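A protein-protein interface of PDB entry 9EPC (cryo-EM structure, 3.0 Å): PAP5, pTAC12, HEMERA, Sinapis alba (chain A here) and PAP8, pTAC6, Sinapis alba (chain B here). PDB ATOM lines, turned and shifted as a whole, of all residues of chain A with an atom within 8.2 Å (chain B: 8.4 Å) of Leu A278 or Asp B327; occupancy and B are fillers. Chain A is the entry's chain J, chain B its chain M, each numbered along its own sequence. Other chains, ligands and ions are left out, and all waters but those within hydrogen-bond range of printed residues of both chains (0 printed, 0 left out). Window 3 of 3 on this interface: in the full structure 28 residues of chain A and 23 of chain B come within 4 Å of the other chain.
The backbone carbonyl oxygen of Ser B329 is in hydrogen-bond range of the side-chain amino group of Lys A221. OG1 of Thr A279 sits at hydrogen-bond distance from OD1 of Asp B327, at 2.7 Å. The side-chain carboxylate (OE2) of Glu A280 is in hydrogen-bond range of the backbone NH (N) of Asn B332 (2.7 Å). The side-chain hydroxyl of Ser B331 sits at hydrogen-bond distance from the side-chain hydroxyl of Thr A277, at 2.5 Å. N of Leu A278 sits at hydrogen-bond distance from OD2 of Asp B327, at 2.8 Å. The backbone NH (N) of Phe A215 lies within hydrogen-bond range of the backbone carbonyl oxygen (O) of Ser B331 (3.1 Å).
Of the printed residues of chain B, Lys A221 touches Ser B329 (2.8 Å). Of the printed residues of chain B, Leu A260 touches Phe B334. Thr A277 touches just these residues of chain B: Asp B327 (3.3 Å), Val B330 (3.3 Å) and Ser B331 (2.5 Å). Of chain B, only Asp B327 (2.8 Å) comes within 4 Å of Leu A278. Of the printed residues of chain B, Leu A283 touches Leu B322, Asn B332 and Phe B334. Printed residues of chain A within 4 Å of Leu B322: Phe A215 (3.8 Å), Thr A279 (3.8 Å) and Leu A283 (3.98 Å). Asp B327 touches just these residues of chain A: Thr A277, Leu A278 and Thr A279. The nearest residue of chain B that does not touch Leu A278 is Leu B325 (4.3 Å). The nearest residue of chain A that does not touch Asp B327 is Glu A280 (5.7 Å). The nearest printed residue of chain A that does not touch Val B330 is Glu A280 (4.3 Å).
Among the printed residues, pairs that only touch across the chains: Phe A215 with Asn B332 (3.1 Å), Tyr A272 with Asn B332 (3.2 Å), Tyr A272 with Val B330 (3.2 Å), Thr A279 with Ser B331 (3.2 Å), Thr A277 with Asp B327 (3.3 Å), Glu A280 with Phe B334 (3.3 Å), Ile A216 with Ser B329 (3.3 Å), Thr A277 with Val B330 (3.3 Å), Thr A279 with Leu B325 (3.4 Å), Glu A280 with Ser B331 (3.4 Å), Phe A215 with Phe B328 (3.4 Å), Leu A283 with Phe B334 (3.5 Å), Leu A260 with Phe B334 (3.7 Å), Phe A215 with Leu B322 (3.8 Å), Thr A279 with Phe B328 (3.8 Å), Thr A279 with Leu B322 (3.8 Å), Tyr A272 with Ser B331 (3.8 Å), Leu A283 with Asn B332 (3.9 Å), Ile A216 with Phe B328 (3.98 Å), Leu A283 with Leu B322 (3.98 Å) and Tyr A284 with Phe B334 (3.99 Å).
The backbone NH (N) of Thr A277 is in hydrogen-bond range of the side-chain carboxylate (OE1) of Glu A280 (3.0 Å). O of Asp B327 sits at hydrogen-bond distance from OG of Ser B331, 2.5 Å away. NZ of Lys A221 lies within hydrogen-bond range of OH of Tyr A272. N of Tyr A272 lies within hydrogen-bond range of OE2 of Glu A280, at 3.1 Å. O of Leu A278 is in hydrogen-bond range of OG of Ser A282 (2.6 Å). The backbone carbonyl oxygen of Thr A277 lies close to the side-chain hydroxyl of Thr A281 (3.5 Å).
Of the 12 printed residues of chain B, 9 touch a printed residue of chain A. Hydrophobic or aromatic side chains of chain B within 4 Å of the printed part of chain A: Leu B322, Leu B325, Phe B328, Val B330 and Phe B334. Along chain B the printed residues that touch a printed residue of chain A span positions 322 to 334.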
ATOM      1  N   PHE A 215      -0.186 -21.252  -9.020  1.00  0.00           N
ATOM      2  CA  PHE A 215      -0.804 -21.769 -10.236  1.00  0.00           C
ATOM      3  C   PHE A 215      -1.549 -23.067  -9.966  1.00  0.00           C
ATOM      4  O   PHE A 215      -2.620 -23.309 -10.535  1.00  0.00           O
ATOM      5  CB  PHE A 215       0.252 -21.976 -11.318  1.00  0.00           C
ATOM      6  CG  PHE A 215       0.470 -20.777 -12.184  1.00  0.00           C
ATOM      7  CD1 PHE A 215      -0.517 -20.346 -13.049  1.00  0.00           C
ATOM      8  CD2 PHE A 215       1.666 -20.087 -12.144  1.00  0.00           C
ATOM      9  CE1 PHE A 215      -0.318 -19.245 -13.852  1.00  0.00           C
ATOM     10  CE2 PHE A 215       1.870 -18.987 -12.945  1.00  0.00           C
ATOM     11  CZ  PHE A 215       0.879 -18.564 -13.799  1.00  0.00           C
ATOM     12  N   ILE A 216      -1.000 -23.915  -9.105  1.00  0.00           N
ATOM     13  CA  ILE A 216      -1.604 -25.190  -8.747  1.00  0.00           C
ATOM     14  C   ILE A 216      -2.056 -25.113  -7.298  1.00  0.00           C
ATOM     15  O   ILE A 216      -1.290 -24.687  -6.426  1.00  0.00           O
ATOM     16  CB  ILE A 216      -0.625 -26.355  -8.963  1.00  0.00           C
ATOM     17  CG1 ILE A 216      -0.134 -26.364 -10.410  1.00  0.00           C
ATOM     18  CG2 ILE A 216      -1.286 -27.675  -8.619  1.00  0.00           C
ATOM     19  CD1 ILE A 216       0.802 -27.498 -10.730  1.00  0.00           C
ATOM     20  N   LYS A 221      -2.534 -30.495  -5.005  1.00  0.00           N
ATOM     21  CA  LYS A 221      -1.245 -30.853  -5.586  1.00  0.00           C
ATOM     22  C   LYS A 221      -0.879 -32.259  -5.129  1.00  0.00           C
ATOM     23  O   LYS A 221      -0.513 -32.467  -3.968  1.00  0.00           O
ATOM     24  CB  LYS A 221      -0.171 -29.846  -5.184  1.00  0.00           C
ATOM     25  CG  LYS A 221       1.227 -30.237  -5.622  1.00  0.00           C
ATOM     26  CD  LYS A 221       2.242 -29.160  -5.288  1.00  0.00           C
ATOM     27  CE  LYS A 221       2.028 -27.918  -6.134  1.00  0.00           C
ATOM     28  NZ  LYS A 221       3.077 -26.894  -5.884  1.00  0.00           N
ATOM     29  N   ARG A 251      21.151 -19.041 -12.933  1.00  0.00           N
ATOM     30  CA  ARG A 251      20.061 -18.426 -13.674  1.00  0.00           C
ATOM     31  C   ARG A 251      20.483 -17.048 -14.167  1.00  0.00           C
ATOM     32  O   ARG A 251      21.143 -16.292 -13.451  1.00  0.00           O
ATOM     33  CB  ARG A 251      18.811 -18.325 -12.805  1.00  0.00           C
ATOM     34  CG  ARG A 251      17.535 -18.135 -13.605  1.00  0.00           C
ATOM     35  CD  ARG A 251      16.307 -18.504 -12.797  1.00  0.00           C
ATOM     36  NE  ARG A 251      16.091 -17.597 -11.678  1.00  0.00           N
ATOM     37  CZ  ARG A 251      15.389 -16.474 -11.752  1.00  0.00           C
ATOM     38  NH1 ARG A 251      14.827 -16.085 -12.883  1.00  0.00           N
ATOM     39  NH2 ARG A 251      15.247 -15.725 -10.664  1.00  0.00           N
ATOM     40  N   ARG A 252      20.111 -16.733 -15.399  1.00  0.00           N
ATOM     41  CA  ARG A 252      20.574 -15.500 -16.021  1.00  0.00           C
ATOM     42  C   ARG A 252      19.971 -14.293 -15.312  1.00  0.00           C
ATOM     43  O   ARG A 252      18.762 -14.272 -15.057  1.00  0.00           O
ATOM     44  CB  ARG A 252      20.206 -15.473 -17.500  1.00  0.00           C
ATOM     45  CG  ARG A 252      21.033 -14.500 -18.318  1.00  0.00           C
ATOM     46  CD  ARG A 252      20.526 -14.392 -19.742  1.00  0.00           C
ATOM     47  NE  ARG A 252      19.389 -13.487 -19.847  1.00  0.00           N
ATOM     48  CZ  ARG A 252      19.486 -12.199 -20.146  1.00  0.00           C
ATOM     49  NH1 ARG A 252      20.656 -11.632 -20.385  1.00  0.00           N
ATOM     50  NH2 ARG A 252      18.381 -11.462 -20.205  1.00  0.00           N
ATOM     51  N   PRO A 253      20.772 -13.288 -14.964  1.00  0.00           N
ATOM     52  CA  PRO A 253      20.207 -12.071 -14.372  1.00  0.00           C
ATOM     53  C   PRO A 253      19.277 -11.377 -15.353  1.00  0.00           C
ATOM     54  O   PRO A 253      19.548 -11.307 -16.552  1.00  0.00           O
ATOM     55  CB  PRO A 253      21.444 -11.217 -14.068  1.00  0.00           C
ATOM     56  CG  PRO A 253      22.589 -12.172 -14.082  1.00  0.00           C
ATOM     57  CD  PRO A 253      22.236 -13.220 -15.076  1.00  0.00           C
ATOM     58  N   ASP A 254      18.174 -10.850 -14.828  1.00  0.00           N
ATOM     59  CA  ASP A 254      17.144 -10.246 -15.657  1.00  0.00           C
ATOM     60  C   ASP A 254      16.607  -8.999 -14.977  1.00  0.00           C
ATOM     61  O   ASP A 254      16.673  -8.852 -13.756  1.00  0.00           O
ATOM     62  CB  ASP A 254      15.989 -11.218 -15.928  1.00  0.00           C
ATOM     63  CG  ASP A 254      16.235 -12.099 -17.132  1.00  0.00           C
ATOM     64  OD1 ASP A 254      17.165 -11.802 -17.911  1.00  0.00           O
ATOM     65  OD2 ASP A 254      15.496 -13.090 -17.303  1.00  0.00           O
ATOM     66  N   GLU A 256      13.443  -8.498 -15.051  1.00  0.00           N
ATOM     67  CA  GLU A 256      12.220  -9.007 -14.442  1.00  0.00           C
ATOM     68  C   GLU A 256      12.465  -9.505 -13.025  1.00  0.00           C
ATOM     69  O   GLU A 256      11.664  -9.241 -12.124  1.00  0.00           O
ATOM     70  CB  GLU A 256      11.631 -10.123 -15.302  1.00  0.00           C
ATOM     71  CG  GLU A 256      11.223  -9.688 -16.695  1.00  0.00           C
ATOM     72  CD  GLU A 256      12.380  -9.675 -17.671  1.00  0.00           C
ATOM     73  OE1 GLU A 256      13.244 -10.571 -17.582  1.00  0.00           O
ATOM     74  OE2 GLU A 256      12.429  -8.766 -18.526  1.00  0.00           O
ATOM     75  N   THR A 257      13.567 -10.226 -12.809  1.00  0.00           N
ATOM     76  CA  THR A 257      13.835 -10.776 -11.484  1.00  0.00           C
ATOM     77  C   THR A 257      14.010  -9.672 -10.451  1.00  0.00           C
ATOM     78  O   THR A 257      13.482  -9.764  -9.338  1.00  0.00           O
ATOM     79  CB  THR A 257      15.079 -11.663 -11.518  1.00  0.00           C
ATOM     80  OG1 THR A 257      16.229 -10.859 -11.803  1.00  0.00           O
ATOM     81  CG2 THR A 257      14.942 -12.723 -12.590  1.00  0.00           C
ATOM     82  N   LEU A 260      10.632  -7.978  -9.877  1.00  0.00           N
ATOM     83  CA  LEU A 260       9.724  -8.900  -9.206  1.00  0.00           C
ATOM     84  C   LEU A 260      10.078  -9.043  -7.733  1.00  0.00           C
ATOM     85  O   LEU A 260       9.189  -9.083  -6.875  1.00  0.00           O
ATOM     86  CB  LEU A 260       9.750 -10.256  -9.907  1.00  0.00           C
ATOM     87  CG  LEU A 260       8.413 -10.974 -10.052  1.00  0.00           C
ATOM     88  CD1 LEU A 260       7.350 -10.011 -10.530  1.00  0.00           C
ATOM     89  CD2 LEU A 260       8.556 -12.127 -11.024  1.00  0.00           C
ATOM     90  N   TYR A 272       5.683 -17.209  -5.275  1.00  0.00           N
ATOM     91  CA  TYR A 272       5.584 -18.522  -4.648  1.00  0.00           C
ATOM     92  C   TYR A 272       6.682 -18.724  -3.612  1.00  0.00           C
ATOM     93  O   TYR A 272       6.440 -19.305  -2.549  1.00  0.00           O
ATOM     94  CB  TYR A 272       5.643 -19.616  -5.711  1.00  0.00           C
ATOM     95  CG  TYR A 272       5.320 -20.998  -5.194  1.00  0.00           C
ATOM     96  CD1 TYR A 272       6.318 -21.827  -4.703  1.00  0.00           C
ATOM     97  CD2 TYR A 272       4.019 -21.475  -5.205  1.00  0.00           C
ATOM     98  CE1 TYR A 272       6.024 -23.090  -4.233  1.00  0.00           C
ATOM     99  CE2 TYR A 272       3.718 -22.735  -4.737  1.00  0.00           C
ATOM    100  CZ  TYR A 272       4.724 -23.538  -4.253  1.00  0.00           C
ATOM    101  OH  TYR A 272       4.426 -24.797  -3.786  1.00  0.00           O
ATOM    102  N   GLU A 275      12.751 -16.556  -4.323  1.00  0.00           N
ATOM    103  CA  GLU A 275      13.302 -16.233  -5.629  1.00  0.00           C
ATOM    104  C   GLU A 275      12.242 -16.386  -6.712  1.00  0.00           C
ATOM    105  O   GLU A 275      11.524 -17.391  -6.740  1.00  0.00           O
ATOM    106  CB  GLU A 275      14.487 -17.144  -5.950  1.00  0.00           C
ATOM    107  CG  GLU A 275      15.321 -16.698  -7.136  1.00  0.00           C
ATOM    108  CD  GLU A 275      16.220 -15.522  -6.806  1.00  0.00           C
ATOM    109  OE1 GLU A 275      16.318 -15.160  -5.615  1.00  0.00           O
ATOM    110  OE2 GLU A 275      16.832 -14.961  -7.739  1.00  0.00           O
ATOM    111  N   PRO A 276      12.114 -15.410  -7.609  1.00  0.00           N
ATOM    112  CA  PRO A 276      11.120 -15.526  -8.683  1.00  0.00           C
ATOM    113  C   PRO A 276      11.533 -16.579  -9.701  1.00  0.00           C
ATOM    114  O   PRO A 276      12.660 -16.577 -10.196  1.00  0.00           O
ATOM    115  CB  PRO A 276      11.101 -14.123  -9.298  1.00  0.00           C
ATOM    116  CG  PRO A 276      12.444 -13.567  -8.991  1.00  0.00           C
ATOM    117  CD  PRO A 276      12.830 -14.125  -7.653  1.00  0.00           C
ATOM    118  N   THR A 277      10.605 -17.479 -10.010  1.00  0.00           N
ATOM    119  CA  THR A 277      10.867 -18.535 -10.972  1.00  0.00           C
ATOM    120  C   THR A 277      10.809 -17.988 -12.395  1.00  0.00           C
ATOM    121  O   THR A 277      10.315 -16.887 -12.647  1.00  0.00           O
ATOM    122  CB  THR A 277       9.865 -19.673 -10.806  1.00  0.00           C
ATOM    123  OG1 THR A 277       8.564 -19.223 -11.197  1.00  0.00           O
ATOM    124  CG2 THR A 277       9.818 -20.126  -9.362  1.00  0.00           C
ATOM    125  N   LEU A 278      11.328 -18.777 -13.337  1.00  0.00           N
ATOM    126  CA  LEU A 278      11.307 -18.362 -14.735  1.00  0.00           C
ATOM    127  C   LEU A 278       9.884 -18.229 -15.258  1.00  0.00           C
ATOM    128  O   LEU A 278       9.628 -17.421 -16.156  1.00  0.00           O
ATOM    129  CB  LEU A 278      12.100 -19.347 -15.590  1.00  0.00           C
ATOM    130  CG  LEU A 278      13.615 -19.251 -15.428  1.00  0.00           C
ATOM    131  CD1 LEU A 278      14.313 -20.236 -16.339  1.00  0.00           C
ATOM    132  CD2 LEU A 278      14.083 -17.838 -15.716  1.00  0.00           C
ATOM    133  N   THR A 279       8.951 -19.015 -14.721  1.00  0.00           N
ATOM    134  CA  THR A 279       7.548 -18.836 -15.074  1.00  0.00           C
ATOM    135  C   THR A 279       7.036 -17.481 -14.606  1.00  0.00           C
ATOM    136  O   THR A 279       6.314 -16.795 -15.338  1.00  0.00           O
ATOM    137  CB  THR A 279       6.708 -19.960 -14.474  1.00  0.00           C
ATOM    138  OG1 THR A 279       7.170 -21.219 -14.976  1.00  0.00           O
ATOM    139  CG2 THR A 279       5.249 -19.786 -14.834  1.00  0.00           C
ATOM    140  N   GLU A 280       7.403 -17.078 -13.390  1.00  0.00           N
ATOM    141  CA  GLU A 280       6.936 -15.803 -12.861  1.00  0.00           C
ATOM    142  C   GLU A 280       7.569 -14.629 -13.596  1.00  0.00           C
ATOM    143  O   GLU A 280       6.903 -13.618 -13.844  1.00  0.00           O
ATOM    144  CB  GLU A 280       7.221 -15.730 -11.363  1.00  0.00           C
ATOM    145  CG  GLU A 280       6.423 -16.743 -10.564  1.00  0.00           C
ATOM    146  CD  GLU A 280       6.891 -16.864  -9.132  1.00  0.00           C
ATOM    147  OE1 GLU A 280       8.030 -16.451  -8.841  1.00  0.00           O
ATOM    148  OE2 GLU A 280       6.119 -17.374  -8.297  1.00  0.00           O
ATOM    149  N   THR A 281       8.852 -14.735 -13.945  1.00  0.00           N
ATOM    150  CA  THR A 281       9.487 -13.671 -14.716  1.00  0.00           C
ATOM    151  C   THR A 281       8.873 -13.559 -16.104  1.00  0.00           C
ATOM    152  O   THR A 281       8.673 -12.451 -16.612  1.00  0.00           O
ATOM    153  CB  THR A 281      10.992 -13.910 -14.817  1.00  0.00           C
ATOM    154  OG1 THR A 281      11.236 -15.138 -15.512  1.00  0.00           O
ATOM    155  CG2 THR A 281      11.607 -13.986 -13.436  1.00  0.00           C
ATOM    156  N   SER A 282       8.577 -14.695 -16.738  1.00  0.00           N
ATOM    157  CA  SER A 282       7.903 -14.664 -18.030  1.00  0.00           C
ATOM    158  C   SER A 282       6.511 -14.068 -17.904  1.00  0.00           C
ATOM    159  O   SER A 282       6.074 -13.300 -18.767  1.00  0.00           O
ATOM    160  CB  SER A 282       7.833 -16.071 -18.617  1.00  0.00           C
ATOM    161  OG  SER A 282       9.103 -16.691 -18.582  1.00  0.00           O
ATOM    162  N   LEU A 283       5.796 -14.418 -16.836  1.00  0.00           N
ATOM    163  CA  LEU A 283       4.491 -13.816 -16.592  1.00  0.00           C
ATOM    164  C   LEU A 283       4.617 -12.326 -16.317  1.00  0.00           C
ATOM    165  O   LEU A 283       3.732 -11.544 -16.681  1.00  0.00           O
ATOM    166  CB  LEU A 283       3.805 -14.521 -15.426  1.00  0.00           C
ATOM    167  CG  LEU A 283       2.463 -13.937 -15.000  1.00  0.00           C
ATOM    168  CD1 LEU A 283       1.503 -13.942 -16.169  1.00  0.00           C
ATOM    169  CD2 LEU A 283       1.903 -14.727 -13.838  1.00  0.00           C
ATOM    170  N   TYR A 284       5.710 -11.913 -15.676  1.00  0.00           N
ATOM    171  CA  TYR A 284       5.896 -10.500 -15.374  1.00  0.00           C
ATOM    172  C   TYR A 284       6.000  -9.672 -16.647  1.00  0.00           C
ATOM    173  O   TYR A 284       5.455  -8.566 -16.716  1.00  0.00           O
ATOM    174  CB  TYR A 284       7.134 -10.302 -14.504  1.00  0.00           C
ATOM    175  CG  TYR A 284       7.467  -8.851 -14.255  1.00  0.00           C
ATOM    176  CD1 TYR A 284       6.679  -8.071 -13.427  1.00  0.00           C
ATOM    177  CD2 TYR A 284       8.572  -8.264 -14.849  1.00  0.00           C
ATOM    178  CE1 TYR A 284       6.981  -6.746 -13.199  1.00  0.00           C
ATOM    179  CE2 TYR A 284       8.881  -6.941 -14.626  1.00  0.00           C
ATOM    180  CZ  TYR A 284       8.084  -6.187 -13.801  1.00  0.00           C
ATOM    181  OH  TYR A 284       8.391  -4.868 -13.577  1.00  0.00           O
ATOM    182  N   ARG A 285       6.687 -10.190 -17.667  1.00  0.00           N
ATOM    183  CA  ARG A 285       6.827  -9.442 -18.913  1.00  0.00           C
ATOM    184  C   ARG A 285       5.473  -9.162 -19.548  1.00  0.00           C
ATOM    185  O   ARG A 285       5.254  -8.082 -20.105  1.00  0.00           O
ATOM    186  CB  ARG A 285       7.719 -10.200 -19.893  1.00  0.00           C
ATOM    187  CG  ARG A 285       9.196 -10.070 -19.616  1.00  0.00           C
ATOM    188  CD  ARG A 285      10.010 -10.510 -20.815  1.00  0.00           C
ATOM    189  NE  ARG A 285       9.671 -11.863 -21.231  1.00  0.00           N
ATOM    190  CZ  ARG A 285      10.250 -12.956 -20.760  1.00  0.00           C
ATOM    191  NH1 ARG A 285      11.208 -12.893 -19.851  1.00  0.00           N
ATOM    192  NH2 ARG A 285       9.860 -14.144 -21.212  1.00  0.00           N
ATOM    193  N   LEU B 322       2.337 -21.146 -20.129  1.00  0.00           N
ATOM    194  CA  LEU B 322       3.295 -21.284 -19.041  1.00  0.00           C
ATOM    195  C   LEU B 322       3.345 -22.694 -18.476  1.00  0.00           C
ATOM    196  O   LEU B 322       4.295 -23.023 -17.759  1.00  0.00           O
ATOM    197  CB  LEU B 322       2.965 -20.302 -17.918  1.00  0.00           C
ATOM    198  CG  LEU B 322       3.091 -18.815 -18.238  1.00  0.00           C
ATOM    199  CD1 LEU B 322       2.697 -17.991 -17.032  1.00  0.00           C
ATOM    200  CD2 LEU B 322       4.502 -18.484 -18.674  1.00  0.00           C
ATOM    201  N   ARG B 323       2.352 -23.531 -18.782  1.00  0.00           N
ATOM    202  CA  ARG B 323       2.299 -24.865 -18.197  1.00  0.00           C
ATOM    203  C   ARG B 323       3.491 -25.715 -18.613  1.00  0.00           C
ATOM    204  O   ARG B 323       3.935 -26.576 -17.845  1.00  0.00           O
ATOM    205  CB  ARG B 323       0.994 -25.555 -18.592  1.00  0.00           C
ATOM    206  CG  ARG B 323       0.788 -26.918 -17.958  1.00  0.00           C
ATOM    207  CD  ARG B 323       0.571 -26.799 -16.462  1.00  0.00           C
ATOM    208  NE  ARG B 323       0.565 -28.094 -15.793  1.00  0.00           N
ATOM    209  CZ  ARG B 323       1.635 -28.662 -15.252  1.00  0.00           C
ATOM    210  NH1 ARG B 323       2.822 -28.080 -15.292  1.00  0.00           N
ATOM    211  NH2 ARG B 323       1.510 -29.844 -14.655  1.00  0.00           N
ATOM    212  N   LYS B 324       4.027 -25.490 -19.810  1.00  0.00           N
ATOM    213  CA  LYS B 324       5.127 -26.304 -20.307  1.00  0.00           C
ATOM    214  C   LYS B 324       6.459 -25.983 -19.644  1.00  0.00           C
ATOM    215  O   LYS B 324       7.424 -26.722 -19.854  1.00  0.00           O
ATOM    216  CB  LYS B 324       5.256 -26.145 -21.822  1.00  0.00           C
ATOM    217  CG  LYS B 324       5.479 -24.721 -22.280  1.00  0.00           C
ATOM    218  CD  LYS B 324       5.426 -24.624 -23.793  1.00  0.00           C
ATOM    219  CE  LYS B 324       5.559 -23.185 -24.259  1.00  0.00           C
ATOM    220  NZ  LYS B 324       5.420 -23.067 -25.736  1.00  0.00           N
ATOM    221  N   LEU B 325       6.545 -24.908 -18.867  1.00  0.00           N
ATOM    222  CA  LEU B 325       7.763 -24.638 -18.117  1.00  0.00           C
ATOM    223  C   LEU B 325       7.858 -25.575 -16.921  1.00  0.00           C
ATOM    224  O   LEU B 325       6.853 -25.896 -16.282  1.00  0.00           O
ATOM    225  CB  LEU B 325       7.796 -23.183 -17.662  1.00  0.00           C
ATOM    226  CG  LEU B 325       7.806 -22.154 -18.792  1.00  0.00           C
ATOM    227  CD1 LEU B 325       7.914 -20.751 -18.236  1.00  0.00           C
ATOM    228  CD2 LEU B 325       8.939 -22.435 -19.758  1.00  0.00           C
ATOM    229  N   ARG B 326       9.077 -26.016 -16.615  1.00  0.00           N
ATOM    230  CA  ARG B 326       9.257 -27.058 -15.613  1.00  0.00           C
ATOM    231  C   ARG B 326       9.217 -26.539 -14.183  1.00  0.00           C
ATOM    232  O   ARG B 326       9.225 -27.350 -13.253  1.00  0.00           O
ATOM    233  CB  ARG B 326      10.570 -27.803 -15.856  1.00  0.00           C
ATOM    234  CG  ARG B 326      11.807 -26.950 -15.748  1.00  0.00           C
ATOM    235  CD  ARG B 326      13.032 -27.747 -16.148  1.00  0.00           C
ATOM    236  NE  ARG B 326      12.914 -28.267 -17.503  1.00  0.00           N
ATOM    237  CZ  ARG B 326      13.853 -28.971 -18.119  1.00  0.00           C
ATOM    238  NH1 ARG B 326      14.998 -29.261 -17.527  1.00  0.00           N
ATOM    239  NH2 ARG B 326      13.637 -29.393 -19.361  1.00  0.00           N
ATOM    240  N   ASP B 327       9.174 -25.225 -13.977  1.00  0.00           N
ATOM    241  CA  ASP B 327       8.981 -24.654 -12.650  1.00  0.00           C
ATOM    242  C   ASP B 327       7.582 -24.067 -12.496  1.00  0.00           C
ATOM    243  O   ASP B 327       7.362 -23.168 -11.680  1.00  0.00           O
ATOM    244  CB  ASP B 327      10.044 -23.601 -12.351  1.00  0.00           C
ATOM    245  CG  ASP B 327      10.114 -22.522 -13.407  1.00  0.00           C
ATOM    246  OD1 ASP B 327       9.379 -22.618 -14.410  1.00  0.00           O
ATOM    247  OD2 ASP B 327      10.909 -21.575 -13.236  1.00  0.00           O
ATOM    248  N   PHE B 328       6.631 -24.564 -13.287  1.00  0.00           N
ATOM    249  CA  PHE B 328       5.261 -24.066 -13.219  1.00  0.00           C
ATOM    250  C   PHE B 328       4.613 -24.396 -11.881  1.00  0.00           C
ATOM    251  O   PHE B 328       3.885 -23.571 -11.320  1.00  0.00           O
ATOM    252  CB  PHE B 328       4.445 -24.651 -14.369  1.00  0.00           C
ATOM    253  CG  PHE B 328       3.018 -24.197 -14.396  1.00  0.00           C
ATOM    254  CD1 PHE B 328       2.669 -23.015 -15.021  1.00  0.00           C
ATOM    255  CD2 PHE B 328       2.023 -24.959 -13.814  1.00  0.00           C
ATOM    256  CE1 PHE B 328       1.358 -22.599 -15.055  1.00  0.00           C
ATOM    257  CE2 PHE B 328       0.712 -24.545 -13.844  1.00  0.00           C
ATOM    258  CZ  PHE B 328       0.380 -23.366 -14.468  1.00  0.00           C
ATOM    259  N   SER B 329       4.861 -25.597 -11.357  1.00  0.00           N
ATOM    260  CA  SER B 329       4.218 -26.014 -10.116  1.00  0.00           C
ATOM    261  C   SER B 329       4.680 -25.203  -8.915  1.00  0.00           C
ATOM    262  O   SER B 329       3.998 -25.203  -7.886  1.00  0.00           O
ATOM    263  CB  SER B 329       4.477 -27.497  -9.864  1.00  0.00           C
ATOM    264  OG  SER B 329       3.968 -28.289 -10.921  1.00  0.00           O
ATOM    265  N   VAL B 330       5.812 -24.513  -9.019  1.00  0.00           N
ATOM    266  CA  VAL B 330       6.353 -23.748  -7.904  1.00  0.00           C
ATOM    267  C   VAL B 330       6.338 -22.269  -8.255  1.00  0.00           C
ATOM    268  O   VAL B 330       7.210 -21.507  -7.825  1.00  0.00           O
ATOM    269  CB  VAL B 330       7.770 -24.219  -7.541  1.00  0.00           C
ATOM    270  CG1 VAL B 330       7.719 -25.597  -6.915  1.00  0.00           C
ATOM    271  CG2 VAL B 330       8.650 -24.233  -8.773  1.00  0.00           C
ATOM    272  N   SER B 331       5.347 -21.853  -9.036  1.00  0.00           N
ATOM    273  CA  SER B 331       5.208 -20.470  -9.460  1.00  0.00           C
ATOM    274  C   SER B 331       3.834 -19.943  -9.079  1.00  0.00           C
ATOM    275  O   SER B 331       2.866 -20.701  -8.977  1.00  0.00           O
ATOM    276  CB  SER B 331       5.414 -20.333 -10.968  1.00  0.00           C
ATOM    277  OG  SER B 331       6.688 -20.820 -11.349  1.00  0.00           O
ATOM    278  N   ASN B 332       3.760 -18.636  -8.859  1.00  0.00           N
ATOM    279  CA  ASN B 332       2.515 -17.958  -8.537  1.00  0.00           C
ATOM    280  C   ASN B 332       1.977 -17.216  -9.753  1.00  0.00           C
ATOM    281  O   ASN B 332       2.689 -16.969 -10.728  1.00  0.00           O
ATOM    282  CB  ASN B 332       2.711 -16.971  -7.385  1.00  0.00           C
ATOM    283  CG  ASN B 332       2.381 -17.575  -6.041  1.00  0.00           C
ATOM    284  OD1 ASN B 332       2.426 -18.789  -5.866  1.00  0.00           O
ATOM    285  ND2 ASN B 332       2.043 -16.725  -5.081  1.00  0.00           N
ATOM    286  N   PHE B 334       0.093 -13.626 -11.038  1.00  0.00           N
ATOM    287  CA  PHE B 334      -0.096 -12.226 -10.684  1.00  0.00           C
ATOM    288  C   PHE B 334      -0.253 -11.363 -11.925  1.00  0.00           C
ATOM    289  O   PHE B 334      -0.747 -10.240 -11.850  1.00  0.00           O
ATOM    290  CB  PHE B 334       1.071 -11.721  -9.841  1.00  0.00           C
ATOM    291  CG  PHE B 334       2.418 -12.038 -10.416  1.00  0.00           C
ATOM    292  CD1 PHE B 334       3.000 -11.205 -11.353  1.00  0.00           C
ATOM    293  CD2 PHE B 334       3.111 -13.161 -10.007  1.00  0.00           C
ATOM    294  CE1 PHE B 334       4.239 -11.492 -11.877  1.00  0.00           C
ATOM    295  CE2 PHE B 334       4.350 -13.452 -10.528  1.00  0.00           C
ATOM    296  CZ  PHE B 334       4.915 -12.616 -11.464  1.00  0.00           C
